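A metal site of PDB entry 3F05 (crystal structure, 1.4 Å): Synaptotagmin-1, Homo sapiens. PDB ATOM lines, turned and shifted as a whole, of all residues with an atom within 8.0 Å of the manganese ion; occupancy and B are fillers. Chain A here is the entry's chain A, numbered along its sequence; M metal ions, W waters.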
ATOM      1  N   LEU A  49      12.567  21.254   2.226  1.00  0.00           N
ATOM      2  CA  LEU A  49      11.955  22.359   1.480  1.00  0.00           C
ATOM      3  C   LEU A  49      11.230  23.335   2.405  1.00  0.00           C
ATOM      4  O   LEU A  49      10.880  24.438   1.998  1.00  0.00           O
ATOM      5  CB  LEU A  49      10.997  21.849   0.396  1.00  0.00           C
ATOM      6  CG  LEU A  49      11.516  20.885  -0.693  1.00  0.00           C
ATOM      7  CD1 LEU A  49      12.855  21.356  -1.257  1.00  0.00           C
ATOM      8  CD2 LEU A  49      11.647  19.492  -0.148  1.00  0.00           C
ATOM      9  N   ASP A  50      10.994  22.909   3.642  1.00  0.00           N
ATOM     10  CA  ASP A  50      10.306  23.746   4.626  1.00  0.00           C
ATOM     11  C   ASP A  50      11.279  24.214   5.713  1.00  0.00           C
ATOM     12  O   ASP A  50      11.057  25.250   6.353  1.00  0.00           O
ATOM     13  CB  ASP A  50       9.131  22.991   5.252  1.00  0.00           C
ATOM     14  CG  ASP A  50       8.062  22.612   4.228  1.00  0.00           C
ATOM     15  OD1 ASP A  50       8.048  23.199   3.123  1.00  0.00           O
ATOM     16  OD2 ASP A  50       7.241  21.720   4.528  1.00  0.00           O
ATOM     17  N   THR A  54      12.405  20.525   7.652  1.00  0.00           N
ATOM     18  CA  THR A  54      12.143  19.251   6.985  1.00  0.00           C
ATOM     19  C   THR A  54      10.850  19.304   6.200  1.00  0.00           C
ATOM     20  O   THR A  54       9.937  20.086   6.525  1.00  0.00           O
ATOM     21  CB  THR A  54      12.079  18.088   7.980  1.00  0.00           C
ATOM     22  OG1 THR A  54      10.973  18.285   8.867  1.00  0.00           O
ATOM     23  CG2 THR A  54      13.385  17.979   8.787  1.00  0.00           C
ATOM     24  N   SER A  55      10.762  18.438   5.201  1.00  0.00           N
ATOM     25  CA  SER A  55       9.605  18.383   4.333  1.00  0.00           C
ATOM     26  C   SER A  55       8.536  17.440   4.868  1.00  0.00           C
ATOM     27  O   SER A  55       8.737  16.789   5.919  1.00  0.00           O
ATOM     28  CB  SER A  55      10.051  17.938   2.943  1.00  0.00           C
ATOM     29  OG  SER A  55      10.808  16.763   2.994  1.00  0.00           O
ATOM     30  N   ASP A  56       7.398  17.414   4.187  1.00  0.00           N
ATOM     31  CA  ASP A  56       6.265  16.539   4.526  1.00  0.00           C
ATOM     32  C   ASP A  56       6.019  15.609   3.321  1.00  0.00           C
ATOM     33  O   ASP A  56       5.062  15.788   2.565  1.00  0.00           O
ATOM     34  CB  ASP A  56       5.045  17.387   4.819  1.00  0.00           C
ATOM     35  CG  ASP A  56       5.328  18.444   5.817  1.00  0.00           C
ATOM     36  OD1 ASP A  56       5.726  18.105   6.939  1.00  0.00           O
ATOM     37  OD2 ASP A  56       5.204  19.633   5.457  1.00  0.00           O
ATOM     38  N   PRO A  57       6.878  14.615   3.158  1.00  0.00           N
ATOM     39  CA  PRO A  57       6.798  13.797   1.937  1.00  0.00           C
ATOM     40  C   PRO A  57       5.658  12.841   1.795  1.00  0.00           C
ATOM     41  O   PRO A  57       5.187  12.242   2.769  1.00  0.00           O
ATOM     42  CB  PRO A  57       8.114  12.991   1.979  1.00  0.00           C
ATOM     43  CG  PRO A  57       8.459  12.899   3.417  1.00  0.00           C
ATOM     44  CD  PRO A  57       7.995  14.216   4.029  1.00  0.00           C
ATOM     45  N   VAL A  75       0.739  11.127   3.860  1.00  0.00           N
ATOM     46  CA  VAL A  75       1.740  12.156   4.066  1.00  0.00           C
ATOM     47  C   VAL A  75       2.468  11.888   5.398  1.00  0.00           C
ATOM     48  O   VAL A  75       1.822  11.629   6.419  1.00  0.00           O
ATOM     49  CB  VAL A  75       1.098  13.569   4.151  1.00  0.00           C
ATOM     50  CG1 VAL A  75       2.139  14.629   4.508  1.00  0.00           C
ATOM     51  CG2 VAL A  75       0.404  13.910   2.847  1.00  0.00           C
ATOM     52  N   HIS A  76       3.786  11.937   5.371  1.00  0.00           N
ATOM     53  CA  HIS A  76       4.587  11.776   6.575  1.00  0.00           C
ATOM     54  C   HIS A  76       5.138  13.130   6.945  1.00  0.00           C
ATOM     55  O   HIS A  76       5.961  13.701   6.236  1.00  0.00           O
ATOM     56  CB  HIS A  76       5.677  10.747   6.347  1.00  0.00           C
ATOM     57  CG  HIS A  76       5.162   9.355   6.302  1.00  0.00           C
ATOM     58  ND1 HIS A  76       5.379   8.449   7.324  1.00  0.00           N
ATOM     59  CD2 HIS A  76       4.334   8.745   5.417  1.00  0.00           C
ATOM     60  CE1 HIS A  76       4.742   7.320   7.050  1.00  0.00           C
ATOM     61  NE2 HIS A  76       4.095   7.480   5.908  1.00  0.00           N
ATOM     62  N   ARG A  77       4.672  13.643   8.065  1.00  0.00           N
ATOM     63  CA  ARG A  77       5.016  14.988   8.464  1.00  0.00           C
ATOM     64  C   ARG A  77       6.442  15.165   8.979  1.00  0.00           C
ATOM     65  O   ARG A  77       6.958  14.333   9.757  1.00  0.00           O
ATOM     66  CB  ARG A  77       4.038  15.468   9.551  1.00  0.00           C
ATOM     67  CG  ARG A  77       2.566  15.460   9.159  1.00  0.00           C
ATOM     68  CD  ARG A  77       2.304  16.334   7.943  1.00  0.00           C
ATOM     69  NE  ARG A  77       0.922  16.855   7.927  1.00  0.00           N
ATOM     70  CZ  ARG A  77      -0.139  16.183   7.485  1.00  0.00           C
ATOM     71  NH1 ARG A  77      -0.008  14.947   7.041  1.00  0.00           N
ATOM     72  NH2 ARG A  77      -1.336  16.761   7.507  1.00  0.00           N
ATOM     73  N   LYS A  78       7.059  16.254   8.545  1.00  0.00           N
ATOM     74  CA  LYS A  78       8.353  16.688   9.055  1.00  0.00           C
ATOM     75  C   LYS A  78       9.406  15.589   9.166  1.00  0.00           C
ATOM     76  O   LYS A  78       9.927  15.297  10.242  1.00  0.00           O
ATOM     77  CB  LYS A  78       8.160  17.432  10.395  1.00  0.00           C
ATOM     78  CG  LYS A  78       7.301  18.729  10.252  1.00  0.00           C
ATOM     79  CD  LYS A  78       6.795  19.235  11.609  1.00  0.00           C
ATOM     80  CE  LYS A  78       5.734  18.279  12.177  1.00  0.00           C
ATOM     81  NZ  LYS A  78       5.176  18.720  13.482  1.00  0.00           N
ATOM     82  N   TYR A 107       6.535  14.221  -3.362  1.00  0.00           N
ATOM     83  CA  TYR A 107       6.152  15.616  -3.204  1.00  0.00           C
ATOM     84  C   TYR A 107       6.236  16.018  -1.747  1.00  0.00           C
ATOM     85  O   TYR A 107       6.189  15.172  -0.860  1.00  0.00           O
ATOM     86  CB  TYR A 107       4.695  15.835  -3.644  1.00  0.00           C
ATOM     87  CG  TYR A 107       4.457  15.824  -5.131  1.00  0.00           C
ATOM     88  CD1 TYR A 107       4.313  14.625  -5.826  1.00  0.00           C
ATOM     89  CD2 TYR A 107       4.339  17.018  -5.838  1.00  0.00           C
ATOM     90  CE1 TYR A 107       4.070  14.622  -7.182  1.00  0.00           C
ATOM     91  CE2 TYR A 107       4.090  17.021  -7.205  1.00  0.00           C
ATOM     92  CZ  TYR A 107       3.963  15.816  -7.875  1.00  0.00           C
ATOM     93  OH  TYR A 107       3.720  15.813  -9.231  1.00  0.00           O
ATOM     94  N   ASP A 108       6.300  17.323  -1.528  1.00  0.00           N
ATOM     95  CA  ASP A 108       6.316  17.905  -0.197  1.00  0.00           C
ATOM     96  C   ASP A 108       4.937  18.513   0.043  1.00  0.00           C
ATOM     97  O   ASP A 108       4.556  19.521  -0.585  1.00  0.00           O
ATOM     98  CB  ASP A 108       7.402  18.980  -0.127  1.00  0.00           C
ATOM     99  CG  ASP A 108       7.369  19.793   1.153  1.00  0.00           C
ATOM    100  OD1 ASP A 108       6.787  19.318   2.146  1.00  0.00           O
ATOM    101  OD2 ASP A 108       7.919  20.918   1.144  1.00  0.00           O
ATOM    102  N   PHE A 109       4.144  17.873   0.901  1.00  0.00           N
ATOM    103  CA  PHE A 109       2.824  18.378   1.183  1.00  0.00           C
ATOM    104  C   PHE A 109       2.879  19.743   1.860  1.00  0.00           C
ATOM    105  O   PHE A 109       3.657  19.954   2.784  1.00  0.00           O
ATOM    106  CB  PHE A 109       2.052  17.420   2.106  1.00  0.00           C
ATOM    107  CG  PHE A 109       0.720  17.946   2.550  1.00  0.00           C
ATOM    108  CD1 PHE A 109      -0.414  17.729   1.777  1.00  0.00           C
ATOM    109  CD2 PHE A 109       0.604  18.707   3.721  1.00  0.00           C
ATOM    110  CE1 PHE A 109      -1.638  18.238   2.161  1.00  0.00           C
ATOM    111  CE2 PHE A 109      -0.637  19.214   4.111  1.00  0.00           C
ATOM    112  CZ  PHE A 109      -1.741  18.984   3.335  1.00  0.00           C
ATOM    113  N   ASP A 110       2.062  20.671   1.368  1.00  0.00           N
ATOM    114  CA  ASP A 110       1.909  21.992   1.971  1.00  0.00           C
ATOM    115  C   ASP A 110       0.424  22.312   1.934  1.00  0.00           C
ATOM    116  O   ASP A 110      -0.219  22.147   0.904  1.00  0.00           O
ATOM    117  CB  ASP A 110       2.698  23.057   1.195  1.00  0.00           C
ATOM    118  CG  ASP A 110       4.242  22.847   1.244  1.00  0.00           C
ATOM    119  OD1 ASP A 110       4.948  23.562   0.481  1.00  0.00           O
ATOM    120  OD2 ASP A 110       4.736  22.007   2.027  1.00  0.00           O
ATOM    121  N   ARG A 111      -0.147  22.771   3.053  1.00  0.00           N
ATOM    122  CA  ARG A 111      -1.575  23.015   3.068  1.00  0.00           C
ATOM    123  C   ARG A 111      -1.996  24.326   2.402  1.00  0.00           C
ATOM    124  O   ARG A 111      -3.126  24.443   1.937  1.00  0.00           O
ATOM    125  CB  ARG A 111      -2.109  22.983   4.521  1.00  0.00           C
ATOM    126  CG  ARG A 111      -3.616  23.069   4.601  1.00  0.00           C
ATOM    127  CD  ARG A 111      -4.113  22.676   5.979  1.00  0.00           C
ATOM    128  NE  ARG A 111      -3.687  21.322   6.340  1.00  0.00           N
ATOM    129  CZ  ARG A 111      -4.355  20.212   6.038  1.00  0.00           C
ATOM    130  NH1 ARG A 111      -5.496  20.271   5.357  1.00  0.00           N
ATOM    131  NH2 ARG A 111      -3.886  19.036   6.408  1.00  0.00           N
ATOM    132  N   LYS A 114       1.059  25.359  -3.454  1.00  0.00           N
ATOM    133  CA  LYS A 114       1.282  24.194  -4.288  1.00  0.00           C
ATOM    134  C   LYS A 114       2.245  23.258  -3.592  1.00  0.00           C
ATOM    135  O   LYS A 114       3.153  23.693  -2.886  1.00  0.00           O
ATOM    136  CB  LYS A 114       1.871  24.604  -5.626  1.00  0.00           C
ATOM    137  CG  LYS A 114       3.230  25.286  -5.511  1.00  0.00           C
ATOM    138  CD  LYS A 114       4.001  25.299  -6.854  1.00  0.00           C
ATOM    139  CE  LYS A 114       3.236  25.999  -7.979  1.00  0.00           C
ATOM    140  NZ  LYS A 114       1.958  25.305  -8.343  1.00  0.00           N
ATOM    141  N   HIS A 115       2.026  21.975  -3.761  1.00  0.00           N
ATOM    142  CA  HIS A 115       2.929  20.986  -3.221  1.00  0.00           C
ATOM    143  C   HIS A 115       4.136  20.934  -4.138  1.00  0.00           C
ATOM    144  O   HIS A 115       4.009  20.660  -5.338  1.00  0.00           O
ATOM    145  CB  HIS A 115       2.255  19.638  -3.238  1.00  0.00           C
ATOM    146  CG  HIS A 115       1.002  19.575  -2.432  1.00  0.00           C
ATOM    147  ND1 HIS A 115       0.347  18.391  -2.180  1.00  0.00           N
ATOM    148  CD2 HIS A 115       0.333  20.530  -1.741  1.00  0.00           C
ATOM    149  CE1 HIS A 115      -0.717  18.632  -1.437  1.00  0.00           C
ATOM    150  NE2 HIS A 115      -0.740  19.921  -1.144  1.00  0.00           N
ATOM    151  N   ASP A 116       5.311  21.222  -3.582  1.00  0.00           N
ATOM    152  CA  ASP A 116       6.543  21.200  -4.341  1.00  0.00           C
ATOM    153  C   ASP A 116       6.950  19.784  -4.648  1.00  0.00           C
ATOM    154  O   ASP A 116       6.882  18.909  -3.795  1.00  0.00           O
ATOM    155  CB  ASP A 116       7.687  21.842  -3.556  1.00  0.00           C
ATOM    156  CG  ASP A 116       7.532  23.344  -3.401  1.00  0.00           C
ATOM    157  OD1 ASP A 116       6.763  23.940  -4.170  1.00  0.00           O
ATOM    158  OD2 ASP A 116       8.212  23.927  -2.527  1.00  0.00           O
HETATM  159 MN    MN M   1       5.723  20.850   3.564  1.00  0.00          MN
HETATM  160  O   HOH W   1       3.753  22.152   5.083  1.00  0.00           O
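NE2 of His 115 is in hydrogen-bond range of O of Asp 110 (3.1 Å). The side-chain carboxylate of Asp 56 sits at hydrogen-bond distance from the backbone NH of Lys 78, at 2.8 Å. N of Asp 108 is in hydrogen-bond range of O of Asp 116 (2.8 Å).
Of the 18 residues printed, 5 come within 4 Å of the manganese ion.
The manganese ion is bound by OD2 of Asp 50 (2.0 Å), OD2 of Asp 110 (2.2 Å), OD2 of Asp 56 (2.3 Å), OD1 of Asp 108 (2.3 Å) and O of Phe 109 (2.4 Å). The manganese ion has five donor atoms within binding distance. Slightly farther from the manganese ion lies water W1 (2.8 Å).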
